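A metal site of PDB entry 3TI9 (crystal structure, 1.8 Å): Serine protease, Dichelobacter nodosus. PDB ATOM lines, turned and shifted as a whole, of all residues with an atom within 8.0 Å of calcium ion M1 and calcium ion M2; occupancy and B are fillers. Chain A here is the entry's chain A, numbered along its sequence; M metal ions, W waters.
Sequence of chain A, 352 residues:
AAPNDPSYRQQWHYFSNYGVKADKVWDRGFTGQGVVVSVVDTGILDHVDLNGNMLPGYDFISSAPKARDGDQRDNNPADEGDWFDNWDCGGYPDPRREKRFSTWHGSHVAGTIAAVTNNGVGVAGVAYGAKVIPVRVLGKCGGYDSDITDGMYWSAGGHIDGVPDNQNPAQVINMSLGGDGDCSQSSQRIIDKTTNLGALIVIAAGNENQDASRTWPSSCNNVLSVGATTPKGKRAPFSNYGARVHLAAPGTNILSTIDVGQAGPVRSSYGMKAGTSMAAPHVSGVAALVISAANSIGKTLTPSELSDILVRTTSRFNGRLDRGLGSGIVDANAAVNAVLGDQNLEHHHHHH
Four residues have an atom within 4 Å of calcium ion M1: Asp 59, Asp 69, Asp 74 and Asn 76.
Along chain A the residues within 4 Å of calcium ion M1 span positions 59 to 76.
The side-chain carboxylate (OD2) of Asp 59 sits close to the guanidinium group (NH1) of Arg 136, at 3.0 Å.
The backbone NH (N) of Ala 78 sits close to the side-chain amide oxygen (OD1) of Asn 76, at 3.2 Å.
NE2 of Gln 72 sits at hydrogen-bond distance from O of Ser 62 (2.9 Å).
O of Ala 67 is in hydrogen-bond range of NH1 of Arg 136 (2.9 Å).
NH1 of Arg 136 sits close to OD2 of Asp 69, 3.7 Å away.
The side-chain carboxylate (OD1) of Asp 59 lies within hydrogen-bond range of the backbone NH (N) of Ile 61 (3.1 Å).
Merely in contact with calcium ion M2: Ala 67 (3.9 Å).
Within 4 Å of calcium ion M2: Ala 67, Asp 69, Asp 71, Gln 72 and Asp 74.
The nearest printed residue that does not touch calcium ion M2 is Asp 59 (4.2 Å).
Calcium ion M1 is bound by the backbone carbonyl oxygen (O) of Asn 76 (2.4 Å), water W2 (2.4 Å), water W1 (2.4 Å), the side-chain carboxylate (OD2) of Asp 69 (2.4 Å), the side-chain carboxylate (OD2) of Asp 59 (2.4 Å), the side-chain carboxylate (OD2) of Asp 74 (2.5 Å) and the side-chain carboxylate (OD1) of Asp 74 (2.6 Å).
Water W1 lies within hydrogen-bond range of OE2 of Glu 80 (2.7 Å), O of Ala 78 (2.8 Å) and NH1 of Arg 136 (3.2 Å).
Water W3 bridges O of Ile 61 and OD1 of Asp 59.
The backbone carbonyl oxygen (O) of Gln 72 binds calcium ion M2 (2.3 Å).
Calcium ion M2 is bound by OD1 of Asp 71, at 2.4 Å.
OD1 of Asp 74 binds calcium ion M2, 2.4 Å away.
Calcium ion M2 is bound by water W3 (2.4 Å).
The side-chain carboxylate (OD1) of Asp 69 binds calcium ion M2 (2.5 Å).
Calcium ion M2 is bound by OD2 of Asp 69, 2.5 Å away.
Calcium ion M2 is bound by the backbone carbonyl oxygen (O) of Asp 71 (2.5 Å).
Calcium ion M2 has seven donor atoms within binding distance.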
ATOM      1  N   TYR A  58       3.334 -26.922 -28.377  1.00  0.00           N
ATOM      2  CA  TYR A  58       3.477 -26.989 -26.926  1.00  0.00           C
ATOM      3  C   TYR A  58       4.927 -26.815 -26.501  1.00  0.00           C
ATOM      4  O   TYR A  58       5.847 -27.199 -27.215  1.00  0.00           O
ATOM      5  CB  TYR A  58       2.904 -28.295 -26.358  1.00  0.00           C
ATOM      6  CG  TYR A  58       2.393 -28.117 -24.937  1.00  0.00           C
ATOM      7  CD1 TYR A  58       1.124 -27.612 -24.689  1.00  0.00           C
ATOM      8  CD2 TYR A  58       3.200 -28.427 -23.847  1.00  0.00           C
ATOM      9  CE1 TYR A  58       0.654 -27.415 -23.394  1.00  0.00           C
ATOM     10  CE2 TYR A  58       2.748 -28.244 -22.530  1.00  0.00           C
ATOM     11  CZ  TYR A  58       1.471 -27.736 -22.324  1.00  0.00           C
ATOM     12  OH  TYR A  58       1.010 -27.551 -21.048  1.00  0.00           O
ATOM     13  N   ASP A  59       5.117 -26.211 -25.321  1.00  0.00           N
ATOM     14  CA  ASP A  59       6.439 -25.970 -24.750  1.00  0.00           C
ATOM     15  C   ASP A  59       6.676 -26.995 -23.658  1.00  0.00           C
ATOM     16  O   ASP A  59       6.120 -26.898 -22.555  1.00  0.00           O
ATOM     17  CB  ASP A  59       6.514 -24.543 -24.197  1.00  0.00           C
ATOM     18  CG  ASP A  59       7.934 -24.102 -23.867  1.00  0.00           C
ATOM     19  OD1 ASP A  59       8.800 -24.957 -23.516  1.00  0.00           O
ATOM     20  OD2 ASP A  59       8.174 -22.879 -23.930  1.00  0.00           O
ATOM     21  N   PHE A  60       7.524 -27.970 -23.953  1.00  0.00           N
ATOM     22  CA  PHE A  60       7.840 -29.042 -23.010  1.00  0.00           C
ATOM     23  C   PHE A  60       9.038 -28.755 -22.100  1.00  0.00           C
ATOM     24  O   PHE A  60       9.375 -29.589 -21.252  1.00  0.00           O
ATOM     25  CB  PHE A  60       8.019 -30.358 -23.758  1.00  0.00           C
ATOM     26  CG  PHE A  60       6.721 -30.997 -24.163  1.00  0.00           C
ATOM     27  CD1 PHE A  60       6.104 -31.925 -23.331  1.00  0.00           C
ATOM     28  CD2 PHE A  60       6.087 -30.641 -25.356  1.00  0.00           C
ATOM     29  CE1 PHE A  60       4.893 -32.506 -23.693  1.00  0.00           C
ATOM     30  CE2 PHE A  60       4.868 -31.211 -25.722  1.00  0.00           C
ATOM     31  CZ  PHE A  60       4.272 -32.147 -24.881  1.00  0.00           C
ATOM     32  N   ILE A  61       9.669 -27.590 -22.238  1.00  0.00           N
ATOM     33  CA  ILE A  61      10.803 -27.250 -21.375  1.00  0.00           C
ATOM     34  C   ILE A  61      10.310 -27.116 -19.914  1.00  0.00           C
ATOM     35  O   ILE A  61       9.502 -26.246 -19.603  1.00  0.00           O
ATOM     36  CB  ILE A  61      11.585 -25.997 -21.851  1.00  0.00           C
ATOM     37  CG1 ILE A  61      12.009 -26.151 -23.323  1.00  0.00           C
ATOM     38  CG2 ILE A  61      12.814 -25.760 -20.958  1.00  0.00           C
ATOM     39  CD1 ILE A  61      12.563 -24.863 -23.978  1.00  0.00           C
ATOM     40  N   SER A  62      10.805 -28.023 -19.054  1.00  0.00           N
ATOM     41  CA  SER A  62      10.389 -28.108 -17.657  1.00  0.00           C
ATOM     42  C   SER A  62      11.041 -27.049 -16.750  1.00  0.00           C
ATOM     43  O   SER A  62      10.476 -26.693 -15.708  1.00  0.00           O
ATOM     44  CB  SER A  62      10.673 -29.503 -17.099  1.00  0.00           C
ATOM     45  OG  SER A  62       9.910 -30.485 -17.787  1.00  0.00           O
ATOM     46  N   SER A  63      12.214 -26.570 -17.159  1.00  0.00           N
ATOM     47  CA  SER A  63      12.949 -25.568 -16.404  1.00  0.00           C
ATOM     48  C   SER A  63      12.568 -24.165 -16.870  1.00  0.00           C
ATOM     49  O   SER A  63      12.812 -23.799 -18.018  1.00  0.00           O
ATOM     50  CB  SER A  63      14.451 -25.766 -16.586  1.00  0.00           C
ATOM     51  OG  SER A  63      15.162 -24.590 -16.228  1.00  0.00           O
ATOM     52  N   ALA A  64      11.979 -23.388 -15.966  1.00  0.00           N
ATOM     53  CA  ALA A  64      11.598 -22.004 -16.271  1.00  0.00           C
ATOM     54  C   ALA A  64      12.789 -21.116 -16.693  1.00  0.00           C
ATOM     55  O   ALA A  64      12.683 -20.419 -17.703  1.00  0.00           O
ATOM     56  CB  ALA A  64      10.843 -21.370 -15.100  1.00  0.00           C
ATOM     57  N   PRO A  65      13.916 -21.146 -15.933  1.00  0.00           N
ATOM     58  CA  PRO A  65      15.070 -20.334 -16.338  1.00  0.00           C
ATOM     59  C   PRO A  65      15.590 -20.666 -17.735  1.00  0.00           C
ATOM     60  O   PRO A  65      15.955 -19.769 -18.486  1.00  0.00           O
ATOM     61  CB  PRO A  65      16.128 -20.671 -15.270  1.00  0.00           C
ATOM     62  CG  PRO A  65      15.345 -21.136 -14.098  1.00  0.00           C
ATOM     63  CD  PRO A  65      14.182 -21.876 -14.672  1.00  0.00           C
ATOM     64  N   LYS A  66      15.613 -21.959 -18.084  1.00  0.00           N
ATOM     65  CA  LYS A  66      16.095 -22.388 -19.385  1.00  0.00           C
ATOM     66  C   LYS A  66      15.136 -22.052 -20.533  1.00  0.00           C
ATOM     67  O   LYS A  66      15.560 -21.829 -21.673  1.00  0.00           O
ATOM     68  CB  LYS A  66      16.450 -23.881 -19.367  1.00  0.00           C
ATOM     69  CG  LYS A  66      17.712 -24.148 -18.544  1.00  0.00           C
ATOM     70  CD  LYS A  66      18.160 -25.587 -18.605  1.00  0.00           C
ATOM     71  CE  LYS A  66      19.493 -25.748 -17.873  1.00  0.00           C
ATOM     72  NZ  LYS A  66      19.869 -27.176 -17.656  1.00  0.00           N
ATOM     73  N   ALA A  67      13.837 -21.995 -20.215  1.00  0.00           N
ATOM     74  CA  ALA A  67      12.804 -21.621 -21.185  1.00  0.00           C
ATOM     75  C   ALA A  67      12.677 -20.119 -21.391  1.00  0.00           C
ATOM     76  O   ALA A  67      12.111 -19.679 -22.395  1.00  0.00           O
ATOM     77  CB  ALA A  67      11.457 -22.216 -20.755  1.00  0.00           C
ATOM     78  N   ARG A  68      13.193 -19.333 -20.434  1.00  0.00           N
ATOM     79  CA  ARG A  68      13.206 -17.858 -20.505  1.00  0.00           C
ATOM     80  C   ARG A  68      11.808 -17.238 -20.687  1.00  0.00           C
ATOM     81  O   ARG A  68      11.669 -16.203 -21.353  1.00  0.00           O
ATOM     82  CB  ARG A  68      14.178 -17.370 -21.593  1.00  0.00           C
ATOM     83  CG  ARG A  68      15.645 -17.521 -21.218  1.00  0.00           C
ATOM     84  CD  ARG A  68      16.526 -17.069 -22.355  1.00  0.00           C
ATOM     85  NE  ARG A  68      17.885 -16.754 -21.908  1.00  0.00           N
ATOM     86  CZ  ARG A  68      18.998 -17.237 -22.460  1.00  0.00           C
ATOM     87  NH1 ARG A  68      18.956 -18.075 -23.490  1.00  0.00           N
ATOM     88  NH2 ARG A  68      20.169 -16.850 -21.961  1.00  0.00           N
ATOM     89  N   ASP A  69      10.801 -17.867 -20.098  1.00  0.00           N
ATOM     90  CA  ASP A  69       9.417 -17.418 -20.239  1.00  0.00           C
ATOM     91  C   ASP A  69       8.660 -17.369 -18.912  1.00  0.00           C
ATOM     92  O   ASP A  69       7.438 -17.226 -18.880  1.00  0.00           O
ATOM     93  CB  ASP A  69       8.677 -18.288 -21.270  1.00  0.00           C
ATOM     94  CG  ASP A  69       8.618 -19.738 -20.876  1.00  0.00           C
ATOM     95  OD1 ASP A  69       8.986 -20.070 -19.724  1.00  0.00           O
ATOM     96  OD2 ASP A  69       8.199 -20.573 -21.711  1.00  0.00           O
ATOM     97  N   GLY A  70       9.397 -17.516 -17.809  1.00  0.00           N
ATOM     98  CA  GLY A  70       8.845 -17.347 -16.460  1.00  0.00           C
ATOM     99  C   GLY A  70       8.007 -18.485 -15.893  1.00  0.00           C
ATOM    100  O   GLY A  70       7.536 -18.404 -14.760  1.00  0.00           O
ATOM    101  N   ASP A  71       7.816 -19.557 -16.672  1.00  0.00           N
ATOM    102  CA  ASP A  71       7.080 -20.720 -16.181  1.00  0.00           C
ATOM    103  C   ASP A  71       7.643 -22.053 -16.686  1.00  0.00           C
ATOM    104  O   ASP A  71       8.536 -22.075 -17.535  1.00  0.00           O
ATOM    105  CB  ASP A  71       5.557 -20.599 -16.447  1.00  0.00           C
ATOM    106  CG  ASP A  71       5.209 -20.523 -17.930  1.00  0.00           C
ATOM    107  OD1 ASP A  71       6.081 -20.756 -18.809  1.00  0.00           O
ATOM    108  OD2 ASP A  71       4.039 -20.226 -18.237  1.00  0.00           O
ATOM    109  N   GLN A  72       7.120 -23.152 -16.165  1.00  0.00           N
ATOM    110  CA  GLN A  72       7.547 -24.471 -16.600  1.00  0.00           C
ATOM    111  C   GLN A  72       6.828 -24.826 -17.906  1.00  0.00           C
ATOM    112  O   GLN A  72       6.716 -23.980 -18.812  1.00  0.00           O
ATOM    113  CB  GLN A  72       7.339 -25.509 -15.499  1.00  0.00           C
ATOM    114  CG  GLN A  72       8.143 -25.232 -14.234  1.00  0.00           C
ATOM    115  CD  GLN A  72       8.075 -26.379 -13.248  1.00  0.00           C
ATOM    116  OE1 GLN A  72       7.107 -26.513 -12.502  1.00  0.00           O
ATOM    117  NE2 GLN A  72       9.113 -27.200 -13.224  1.00  0.00           N
ATOM    118  N   ARG A  73       6.331 -26.048 -18.045  1.00  0.00           N
ATOM    119  CA  ARG A  73       5.666 -26.429 -19.293  1.00  0.00           C
ATOM    120  C   ARG A  73       4.435 -25.571 -19.526  1.00  0.00           C
ATOM    121  O   ARG A  73       3.719 -25.221 -18.574  1.00  0.00           O
ATOM    122  CB  ARG A  73       5.348 -27.927 -19.321  1.00  0.00           C
ATOM    123  CG  ARG A  73       6.594 -28.805 -19.394  1.00  0.00           C
ATOM    124  CD  ARG A  73       6.224 -30.278 -19.503  1.00  0.00           C
ATOM    125  NE  ARG A  73       7.395 -31.102 -19.804  1.00  0.00           N
ATOM    126  CZ  ARG A  73       7.379 -32.427 -19.854  1.00  0.00           C
ATOM    127  NH1 ARG A  73       6.253 -33.094 -19.614  1.00  0.00           N
ATOM    128  NH2 ARG A  73       8.496 -33.095 -20.140  1.00  0.00           N
ATOM    129  N   ASP A  74       4.216 -25.191 -20.778  1.00  0.00           N
ATOM    130  CA  ASP A  74       3.138 -24.265 -21.156  1.00  0.00           C
ATOM    131  C   ASP A  74       2.735 -24.433 -22.620  1.00  0.00           C
ATOM    132  O   ASP A  74       3.432 -25.097 -23.400  1.00  0.00           O
ATOM    133  CB  ASP A  74       3.573 -22.821 -20.890  1.00  0.00           C
ATOM    134  CG  ASP A  74       4.681 -22.381 -21.821  1.00  0.00           C
ATOM    135  OD1 ASP A  74       5.866 -22.425 -21.426  1.00  0.00           O
ATOM    136  OD2 ASP A  74       4.373 -21.988 -22.960  1.00  0.00           O
ATOM    137  N   ASN A  75       1.623 -23.812 -23.003  1.00  0.00           N
ATOM    138  CA  ASN A  75       1.061 -23.970 -24.349  1.00  0.00           C
ATOM    139  C   ASN A  75       1.565 -22.973 -25.395  1.00  0.00           C
ATOM    140  O   ASN A  75       0.952 -22.833 -26.454  1.00  0.00           O
ATOM    141  CB  ASN A  75      -0.469 -23.952 -24.280  1.00  0.00           C
ATOM    142  CG  ASN A  75      -1.009 -22.634 -23.744  1.00  0.00           C
ATOM    143  OD1 ASN A  75      -0.323 -21.608 -23.741  1.00  0.00           O
ATOM    144  ND2 ASN A  75      -2.260 -22.652 -23.281  1.00  0.00           N
ATOM    145  N   ASN A  76       2.651 -22.271 -25.078  1.00  0.00           N
ATOM    146  CA  ASN A  76       3.239 -21.288 -25.988  1.00  0.00           C
ATOM    147  C   ASN A  76       4.669 -21.683 -26.366  1.00  0.00           C
ATOM    148  O   ASN A  76       5.619 -21.366 -25.635  1.00  0.00           O
ATOM    149  CB  ASN A  76       3.219 -19.884 -25.349  1.00  0.00           C
ATOM    150  CG  ASN A  76       3.773 -18.798 -26.290  1.00  0.00           C
ATOM    151  OD1 ASN A  76       4.063 -19.053 -27.457  1.00  0.00           O
ATOM    152  ND2 ASN A  76       3.928 -17.590 -25.768  1.00  0.00           N
ATOM    153  N   PRO A  77       4.835 -22.382 -27.501  1.00  0.00           N
ATOM    154  CA  PRO A  77       6.170 -22.825 -27.928  1.00  0.00           C
ATOM    155  C   PRO A  77       7.015 -21.713 -28.563  1.00  0.00           C
ATOM    156  O   PRO A  77       7.834 -21.988 -29.443  1.00  0.00           O
ATOM    157  CB  PRO A  77       5.849 -23.913 -28.951  1.00  0.00           C
ATOM    158  CG  PRO A  77       4.576 -23.426 -29.595  1.00  0.00           C
ATOM    159  CD  PRO A  77       3.788 -22.802 -28.454  1.00  0.00           C
ATOM    160  N   ALA A  78       6.856 -20.465 -28.109  1.00  0.00           N
ATOM    161  CA  ALA A  78       7.688 -19.383 -28.625  1.00  0.00           C
ATOM    162  C   ALA A  78       9.169 -19.623 -28.299  1.00  0.00           C
ATOM    163  O   ALA A  78       9.515 -19.986 -27.175  1.00  0.00           O
ATOM    164  CB  ALA A  78       7.239 -18.032 -28.065  1.00  0.00           C
ATOM    165  N   ASP A  79      10.019 -19.459 -29.310  1.00  0.00           N
ATOM    166  CA  ASP A  79      11.467 -19.492 -29.077  1.00  0.00           C
ATOM    167  C   ASP A  79      11.909 -18.134 -28.505  1.00  0.00           C
ATOM    168  O   ASP A  79      11.882 -17.119 -29.192  1.00  0.00           O
ATOM    169  CB  ASP A  79      12.238 -19.825 -30.362  1.00  0.00           C
ATOM    170  CG  ASP A  79      13.722 -20.135 -30.111  1.00  0.00           C
ATOM    171  OD1 ASP A  79      14.199 -19.995 -28.965  1.00  0.00           O
ATOM    172  OD2 ASP A  79      14.405 -20.512 -31.084  1.00  0.00           O
ATOM    173  N   GLU A  80      12.301 -18.148 -27.222  1.00  0.00           N
ATOM    174  CA  GLU A  80      12.735 -16.936 -26.521  1.00  0.00           C
ATOM    175  C   GLU A  80      14.219 -16.645 -26.749  1.00  0.00           C
ATOM    176  O   GLU A  80      14.745 -15.616 -26.302  1.00  0.00           O
ATOM    177  CB  GLU A  80      12.456 -17.062 -25.013  1.00  0.00           C
ATOM    178  CG  GLU A  80      11.057 -17.579 -24.655  1.00  0.00           C
ATOM    179  CD  GLU A  80       9.943 -16.585 -24.952  1.00  0.00           C
ATOM    180  OE1 GLU A  80      10.251 -15.408 -25.263  1.00  0.00           O
ATOM    181  OE2 GLU A  80       8.753 -16.989 -24.858  1.00  0.00           O
ATOM    182  N   ARG A 136       8.384 -27.336 -28.582  1.00  0.00           N
ATOM    183  CA  ARG A 136       9.584 -26.739 -27.988  1.00  0.00           C
ATOM    184  C   ARG A 136      10.140 -27.596 -26.860  1.00  0.00           C
ATOM    185  O   ARG A 136       9.476 -27.823 -25.840  1.00  0.00           O
ATOM    186  CB  ARG A 136       9.288 -25.310 -27.513  1.00  0.00           C
ATOM    187  CG  ARG A 136      10.548 -24.565 -27.065  1.00  0.00           C
ATOM    188  CD  ARG A 136      10.235 -23.196 -26.487  1.00  0.00           C
ATOM    189  NE  ARG A 136      11.450 -22.402 -26.285  1.00  0.00           N
ATOM    190  CZ  ARG A 136      11.635 -21.535 -25.285  1.00  0.00           C
ATOM    191  NH1 ARG A 136      10.712 -21.364 -24.353  1.00  0.00           N
ATOM    192  NH2 ARG A 136      12.771 -20.850 -25.222  1.00  0.00           N
HETATM  193 CA    CA M   1       6.637 -21.030 -23.510  1.00  0.00          CA
HETATM  194 CA    CA M   2       7.635 -22.172 -19.869  1.00  0.00          CA
HETATM  195  O   HOH W   1       8.063 -19.562 -24.798  1.00  0.00           O
HETATM  196  O   HOH W   2       5.444 -19.092 -22.779  1.00  0.00           O
HETATM  197  O   HOH W   3       8.882 -24.006 -20.810  1.00  0.00           O
